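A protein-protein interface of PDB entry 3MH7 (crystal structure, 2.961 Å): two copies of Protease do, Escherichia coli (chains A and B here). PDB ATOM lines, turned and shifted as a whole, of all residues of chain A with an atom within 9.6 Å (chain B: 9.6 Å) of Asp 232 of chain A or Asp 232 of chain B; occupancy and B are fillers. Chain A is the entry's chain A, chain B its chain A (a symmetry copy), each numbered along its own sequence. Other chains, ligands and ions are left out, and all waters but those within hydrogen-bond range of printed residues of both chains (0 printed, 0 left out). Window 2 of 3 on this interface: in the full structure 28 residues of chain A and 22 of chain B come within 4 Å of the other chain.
The side-chain amide nitrogen of Asn 206 of chain A sits at hydrogen-bond distance from the backbone carbonyl oxygen of Ile 236 of chain B (3.1 Å). OD2 of Asp 232 of chain B sits close to OD2 of Asp 232 of chain A, at 3.4 Å.
Hydrophobic or aromatic side chains of chain B that line the printed part of chain A: Leu 229 and Ile 236. Along chain B the printed residues that touch a printed residue of chain A span positions 229 to 236. Hydrophobic or aromatic side chains of chain A that line the printed part of chain B: Phe 171. Among the printed residues, 6 pairs touch across the chains. Among the printed residues, no Asp or Glu carboxylate lies within 4 Å of a Lys or Arg side-chain nitrogen of the other chain.
Phe 171 of chain A touches Leu 229 of chain B, but with the chains exchanged Leu 229 of chain A does not touch Phe 171 of chain B (18.0 Å). Asn 206 of chain A touches Ile 236 of chain B, but with the chains exchanged Ile 236 of chain A does not touch Asn 206 of chain B (10.4 Å). Asp 232 of chain A touches Pro 231 of chain B, but with the chains exchanged Pro 231 of chain A does not touch Asp 232 of chain B (6.7 Å). Asp 232 of chain A touches its own counterpart, Asp 232 of chain B. Of the 6 pairs that touch across the chains among the printed residues, 1 has its exchanged pair printed and touching as well.
The backbone NH (N) of Phe 171 of chain A sits at hydrogen-bond distance from the backbone carbonyl oxygen (O) of Arg 207 of chain A (2.7 Å). The backbone NH (N) of Asn 235 of chain A lies within hydrogen-bond range of the side-chain amide oxygen (OD1) of Asn 206 of chain A.
Among the printed residues, merely in contact across the chains: Phe 171 of chain A with Leu 229 of chain B, Asp 232 of chain A with Pro 231 of chain B, Gly 234 of chain A with Ile 236 of chain B and Asn 235 of chain A with Ile 236 of chain B.
Pro 231 of chain A touches none of the printed residues of chain B. Asp 232 of chain A touches just these residues of chain B: Pro 231 and Asp 232. No residue of chain B comes within 4 Å of Gly 233 of chain A. Gly 234 of chain A touches just one residue of chain B: Ile 236. Printed residues of chain B within 4 Å of Asn 235 of chain A: Ile 236. Of the printed residues of chain A, Leu 229 of chain B touches Phe 171 (3.6 Å). Of chain A, only Asp 232 comes within 4 Å of Asp 232 of chain B. No residue of chain A comes within 4 Å of Gly 233 of chain B. No residue of chain A comes within 4 Å of Gly 234 of chain B. The nearest residue of chain B that does not touch Asp 232 of chain A is Ile 236 of chain B (6.3 Å). The nearest residue of chain A that does not touch Asp 232 of chain B is Pro 231 of chain A (6.7 Å).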
ATOM      1  N   PHE A 171       7.515   8.265  15.111  1.00  0.00           N
ATOM      2  CA  PHE A 171       6.817   7.162  15.781  1.00  0.00           C
ATOM      3  C   PHE A 171       5.354   7.010  15.319  1.00  0.00           C
ATOM      4  O   PHE A 171       4.486   6.607  16.076  1.00  0.00           O
ATOM      5  CB  PHE A 171       6.865   7.355  17.295  1.00  0.00           C
ATOM      6  CG  PHE A 171       8.244   7.613  17.838  1.00  0.00           C
ATOM      7  CD1 PHE A 171       8.665   8.905  18.125  1.00  0.00           C
ATOM      8  CD2 PHE A 171       9.120   6.570  18.079  1.00  0.00           C
ATOM      9  CE1 PHE A 171       9.950   9.151  18.640  1.00  0.00           C
ATOM     10  CE2 PHE A 171      10.395   6.803  18.590  1.00  0.00           C
ATOM     11  CZ  PHE A 171      10.811   8.099  18.870  1.00  0.00           C
ATOM     12  N   ASN A 206      13.081  12.508  14.835  1.00  0.00           N
ATOM     13  CA  ASN A 206      13.154  11.144  15.344  1.00  0.00           C
ATOM     14  C   ASN A 206      12.706  10.106  14.318  1.00  0.00           C
ATOM     15  O   ASN A 206      12.394  10.458  13.174  1.00  0.00           O
ATOM     16  CB  ASN A 206      12.362  11.007  16.633  1.00  0.00           C
ATOM     17  CG  ASN A 206      12.927  11.863  17.747  1.00  0.00           C
ATOM     18  OD1 ASN A 206      13.874  11.462  18.426  1.00  0.00           O
ATOM     19  ND2 ASN A 206      12.347  13.048  17.943  1.00  0.00           N
ATOM     20  N   ARG A 207      12.701   8.832  14.728  1.00  0.00           N
ATOM     21  CA  ARG A 207      12.340   7.714  13.849  1.00  0.00           C
ATOM     22  C   ARG A 207      10.930   7.937  13.361  1.00  0.00           C
ATOM     23  O   ARG A 207      10.019   8.082  14.166  1.00  0.00           O
ATOM     24  CB  ARG A 207      12.399   6.368  14.587  1.00  0.00           C
ATOM     25  CG  ARG A 207      13.767   5.633  14.578  1.00  0.00           C
ATOM     26  CD  ARG A 207      14.023   4.958  15.948  1.00  0.00           C
ATOM     27  NE  ARG A 207      15.167   4.030  16.014  1.00  0.00           N
ATOM     28  CZ  ARG A 207      16.461   4.349  15.860  1.00  0.00           C
ATOM     29  NH1 ARG A 207      16.848   5.594  15.577  1.00  0.00           N
ATOM     30  NH2 ARG A 207      17.385   3.394  15.967  1.00  0.00           N
ATOM     31  N   ILE A 228      19.980  10.933  12.000  1.00  0.00           N
ATOM     32  CA  ILE A 228      20.318  11.675  13.201  1.00  0.00           C
ATOM     33  C   ILE A 228      21.474  11.061  13.953  1.00  0.00           C
ATOM     34  O   ILE A 228      21.583   9.859  14.065  1.00  0.00           O
ATOM     35  CB  ILE A 228      19.137  11.792  14.173  1.00  0.00           C
ATOM     36  CG1 ILE A 228      18.532  10.429  14.467  1.00  0.00           C
ATOM     37  CG2 ILE A 228      18.077  12.723  13.635  1.00  0.00           C
ATOM     38  CD1 ILE A 228      18.004  10.348  15.867  1.00  0.00           C
ATOM     39  N   LEU A 229      22.347  11.900  14.467  1.00  0.00           N
ATOM     40  CA  LEU A 229      23.300  11.418  15.432  1.00  0.00           C
ATOM     41  C   LEU A 229      22.557  11.281  16.750  1.00  0.00           C
ATOM     42  O   LEU A 229      21.794  12.173  17.152  1.00  0.00           O
ATOM     43  CB  LEU A 229      24.481  12.367  15.566  1.00  0.00           C
ATOM     44  CG  LEU A 229      25.642  11.641  16.246  1.00  0.00           C
ATOM     45  CD1 LEU A 229      25.941  10.358  15.476  1.00  0.00           C
ATOM     46  CD2 LEU A 229      26.875  12.516  16.345  1.00  0.00           C
ATOM     47  N   ALA A 230      22.763  10.155  17.415  1.00  0.00           N
ATOM     48  CA  ALA A 230      21.934   9.807  18.553  1.00  0.00           C
ATOM     49  C   ALA A 230      22.274   8.430  19.087  1.00  0.00           C
ATOM     50  O   ALA A 230      21.917   7.420  18.480  1.00  0.00           O
ATOM     51  CB  ALA A 230      20.470   9.846  18.151  1.00  0.00           C
ATOM     52  N   PRO A 231      22.987   8.386  20.218  1.00  0.00           N
ATOM     53  CA  PRO A 231      23.001   7.170  21.039  1.00  0.00           C
ATOM     54  C   PRO A 231      21.603   6.952  21.610  1.00  0.00           C
ATOM     55  O   PRO A 231      20.957   7.916  22.043  1.00  0.00           O
ATOM     56  CB  PRO A 231      23.962   7.527  22.174  1.00  0.00           C
ATOM     57  CG  PRO A 231      23.975   9.043  22.218  1.00  0.00           C
ATOM     58  CD  PRO A 231      23.831   9.451  20.783  1.00  0.00           C
ATOM     59  N   ASP A 232      21.124   5.717  21.587  1.00  0.00           N
ATOM     60  CA  ASP A 232      19.837   5.413  22.198  1.00  0.00           C
ATOM     61  C   ASP A 232      18.652   5.937  21.384  1.00  0.00           C
ATOM     62  O   ASP A 232      17.617   6.308  21.939  1.00  0.00           O
ATOM     63  CB  ASP A 232      19.799   5.978  23.625  1.00  0.00           C
ATOM     64  CG  ASP A 232      18.663   5.392  24.470  1.00  0.00           C
ATOM     65  OD1 ASP A 232      18.523   4.141  24.529  1.00  0.00           O
ATOM     66  OD2 ASP A 232      17.917   6.193  25.088  1.00  0.00           O
ATOM     67  N   GLY A 233      18.812   5.975  20.067  1.00  0.00           N
ATOM     68  CA  GLY A 233      17.710   6.270  19.159  1.00  0.00           C
ATOM     69  C   GLY A 233      16.729   7.380  19.531  1.00  0.00           C
ATOM     70  O   GLY A 233      15.590   7.387  19.052  1.00  0.00           O
ATOM     71  N   GLY A 234      17.163   8.315  20.375  1.00  0.00           N
ATOM     72  CA  GLY A 234      16.381   9.501  20.682  1.00  0.00           C
ATOM     73  C   GLY A 234      17.125  10.740  20.222  1.00  0.00           C
ATOM     74  O   GLY A 234      18.346  10.770  20.284  1.00  0.00           O
ATOM     75  N   ASN A 235      16.395  11.748  19.748  1.00  0.00           N
ATOM     76  CA  ASN A 235      16.987  12.996  19.265  1.00  0.00           C
ATOM     77  C   ASN A 235      17.748  13.769  20.354  1.00  0.00           C
ATOM     78  O   ASN A 235      17.277  13.890  21.483  1.00  0.00           O
ATOM     79  CB  ASN A 235      15.900  13.871  18.633  1.00  0.00           C
ATOM     80  CG  ASN A 235      16.442  15.178  18.078  1.00  0.00           C
ATOM     81  OD1 ASN A 235      16.674  15.310  16.863  1.00  0.00           O
ATOM     82  ND2 ASN A 235      16.644  16.155  18.957  1.00  0.00           N
ATOM     83  N   ILE A 236      18.933  14.277  20.024  1.00  0.00           N
ATOM     84  CA  ILE A 236      19.702  15.082  20.973  1.00  0.00           C
ATOM     85  C   ILE A 236      20.114  16.448  20.418  1.00  0.00           C
ATOM     86  O   ILE A 236      20.979  17.110  20.987  1.00  0.00           O
ATOM     87  CB  ILE A 236      20.979  14.375  21.448  1.00  0.00           C
ATOM     88  CG1 ILE A 236      21.856  14.022  20.260  1.00  0.00           C
ATOM     89  CG2 ILE A 236      20.658  13.156  22.234  1.00  0.00           C
ATOM     90  CD1 ILE A 236      22.984  13.111  20.586  1.00  0.00           C
ATOM     91  N   PHE B 171      13.570  17.771  37.271  1.00  0.00           N
ATOM     92  CA  PHE B 171      14.522  17.211  38.237  1.00  0.00           C
ATOM     93  C   PHE B 171      14.712  18.105  39.479  1.00  0.00           C
ATOM     94  O   PHE B 171      15.778  18.155  40.070  1.00  0.00           O
ATOM     95  CB  PHE B 171      15.870  16.968  37.562  1.00  0.00           C
ATOM     96  CG  PHE B 171      15.783  16.187  36.280  1.00  0.00           C
ATOM     97  CD1 PHE B 171      15.806  16.833  35.051  1.00  0.00           C
ATOM     98  CD2 PHE B 171      15.693  14.807  36.293  1.00  0.00           C
ATOM     99  CE1 PHE B 171      15.733  16.107  33.849  1.00  0.00           C
ATOM    100  CE2 PHE B 171      15.621  14.078  35.107  1.00  0.00           C
ATOM    101  CZ  PHE B 171      15.640  14.732  33.882  1.00  0.00           C
ATOM    102  N   ASN B 206      10.815  17.613  30.833  1.00  0.00           N
ATOM    103  CA  ASN B 206      11.315  16.421  31.507  1.00  0.00           C
ATOM    104  C   ASN B 206      10.617  16.157  32.839  1.00  0.00           C
ATOM    105  O   ASN B 206       9.688  16.886  33.208  1.00  0.00           O
ATOM    106  CB  ASN B 206      12.821  16.499  31.691  1.00  0.00           C
ATOM    107  CG  ASN B 206      13.559  16.531  30.369  1.00  0.00           C
ATOM    108  OD1 ASN B 206      13.807  15.488  29.763  1.00  0.00           O
ATOM    109  ND2 ASN B 206      13.918  17.733  29.914  1.00  0.00           N
ATOM    110  N   ARG B 207      11.056  15.105  33.539  1.00  0.00           N
ATOM    111  CA  ARG B 207      10.461  14.693  34.816  1.00  0.00           C
ATOM    112  C   ARG B 207      10.586  15.842  35.784  1.00  0.00           C
ATOM    113  O   ARG B 207      11.687  16.321  36.028  1.00  0.00           O
ATOM    114  CB  ARG B 207      11.174  13.469  35.407  1.00  0.00           C
ATOM    115  CG  ARG B 207      10.639  12.078  34.973  1.00  0.00           C
ATOM    116  CD  ARG B 207      11.813  11.087  34.776  1.00  0.00           C
ATOM    117  NE  ARG B 207      11.448   9.671  34.593  1.00  0.00           N
ATOM    118  CZ  ARG B 207      10.759   9.153  33.565  1.00  0.00           C
ATOM    119  NH1 ARG B 207      10.280   9.919  32.584  1.00  0.00           N
ATOM    120  NH2 ARG B 207      10.523   7.841  33.533  1.00  0.00           N
ATOM    121  N   ILE B 228       5.470  12.863  28.190  1.00  0.00           N
ATOM    122  CA  ILE B 228       6.387  12.929  27.066  1.00  0.00           C
ATOM    123  C   ILE B 228       6.625  11.579  26.435  1.00  0.00           C
ATOM    124  O   ILE B 228       6.742  10.580  27.113  1.00  0.00           O
ATOM    125  CB  ILE B 228       7.752  13.512  27.453  1.00  0.00           C
ATOM    126  CG1 ILE B 228       8.337  12.788  28.655  1.00  0.00           C
ATOM    127  CG2 ILE B 228       7.653  14.991  27.739  1.00  0.00           C
ATOM    128  CD1 ILE B 228       9.832  12.719  28.586  1.00  0.00           C
ATOM    129  N   LEU B 229       6.691  11.553  25.121  1.00  0.00           N
ATOM    130  CA  LEU B 229       7.200  10.376  24.467  1.00  0.00           C
ATOM    131  C   LEU B 229       8.713  10.416  24.609  1.00  0.00           C
ATOM    132  O   LEU B 229       9.349  11.461  24.400  1.00  0.00           O
ATOM    133  CB  LEU B 229       6.788  10.333  23.004  1.00  0.00           C
ATOM    134  CG  LEU B 229       6.965   8.912  22.467  1.00  0.00           C
ATOM    135  CD1 LEU B 229       6.205   7.945  23.371  1.00  0.00           C
ATOM    136  CD2 LEU B 229       6.504   8.790  21.029  1.00  0.00           C
ATOM    137  N   ALA B 230       9.289   9.285  24.983  1.00  0.00           N
ATOM    138  CA  ALA B 230      10.683   9.261  25.381  1.00  0.00           C
ATOM    139  C   ALA B 230      11.097   7.889  25.874  1.00  0.00           C
ATOM    140  O   ALA B 230      10.742   7.493  26.985  1.00  0.00           O
ATOM    141  CB  ALA B 230      10.919  10.285  26.478  1.00  0.00           C
ATOM    142  N   PRO B 231      11.835   7.150  25.039  1.00  0.00           N
ATOM    143  CA  PRO B 231      12.635   6.032  25.547  1.00  0.00           C
ATOM    144  C   PRO B 231      13.742   6.591  26.436  1.00  0.00           C
ATOM    145  O   PRO B 231      14.354   7.610  26.092  1.00  0.00           O
ATOM    146  CB  PRO B 231      13.255   5.441  24.279  1.00  0.00           C
ATOM    147  CG  PRO B 231      13.214   6.565  23.260  1.00  0.00           C
ATOM    148  CD  PRO B 231      11.948   7.300  23.579  1.00  0.00           C
ATOM    149  N   ASP B 232      13.980   5.961  27.578  1.00  0.00           N
ATOM    150  CA  ASP B 232      15.081   6.377  28.435  1.00  0.00           C
ATOM    151  C   ASP B 232      14.803   7.693  29.166  1.00  0.00           C
ATOM    152  O   ASP B 232      15.717   8.476  29.431  1.00  0.00           O
ATOM    153  CB  ASP B 232      16.367   6.487  27.604  1.00  0.00           C
ATOM    154  CG  ASP B 232      17.633   6.544  28.465  1.00  0.00           C
ATOM    155  OD1 ASP B 232      17.807   5.674  29.360  1.00  0.00           O
ATOM    156  OD2 ASP B 232      18.463   7.459  28.231  1.00  0.00           O
ATOM    157  N   GLY B 233      13.537   7.936  29.482  1.00  0.00           N
ATOM    158  CA  GLY B 233      13.150   9.049  30.339  1.00  0.00           C
ATOM    159  C   GLY B 233      13.838  10.399  30.145  1.00  0.00           C
ATOM    160  O   GLY B 233      13.871  11.217  31.070  1.00  0.00           O
ATOM    161  N   GLY B 234      14.380  10.636  28.951  1.00  0.00           N
ATOM    162  CA  GLY B 234      14.923  11.937  28.595  1.00  0.00           C
ATOM    163  C   GLY B 234      14.137  12.521  27.437  1.00  0.00           C
ATOM    164  O   GLY B 234      13.689  11.780  26.575  1.00  0.00           O
ATOM    165  N   ASN B 235      13.957  13.841  27.428  1.00  0.00           N
ATOM    166  CA  ASN B 235      13.212  14.531  26.375  1.00  0.00           C
ATOM    167  C   ASN B 235      13.849  14.388  24.984  1.00  0.00           C
ATOM    168  O   ASN B 235      15.065  14.500  24.838  1.00  0.00           O
ATOM    169  CB  ASN B 235      13.041  16.007  26.748  1.00  0.00           C
ATOM    170  CG  ASN B 235      12.247  16.791  25.714  1.00  0.00           C
ATOM    171  OD1 ASN B 235      11.040  17.035  25.885  1.00  0.00           O
ATOM    172  ND2 ASN B 235      12.915  17.193  24.637  1.00  0.00           N
ATOM    173  N   ILE B 236      13.036  14.120  23.966  1.00  0.00           N
ATOM    174  CA  ILE B 236      13.543  14.030  22.597  1.00  0.00           C
ATOM    175  C   ILE B 236      12.801  14.937  21.612  1.00  0.00           C
ATOM    176  O   ILE B 236      12.929  14.768  20.401  1.00  0.00           O
ATOM    177  CB  ILE B 236      13.484  12.600  22.040  1.00  0.00           C
ATOM    178  CG1 ILE B 236      12.059  12.078  22.086  1.00  0.00           C
ATOM    179  CG2 ILE B 236      14.391  11.693  22.788  1.00  0.00           C
ATOM    180  CD1 ILE B 236      11.936  10.622  21.813  1.00  0.00           C
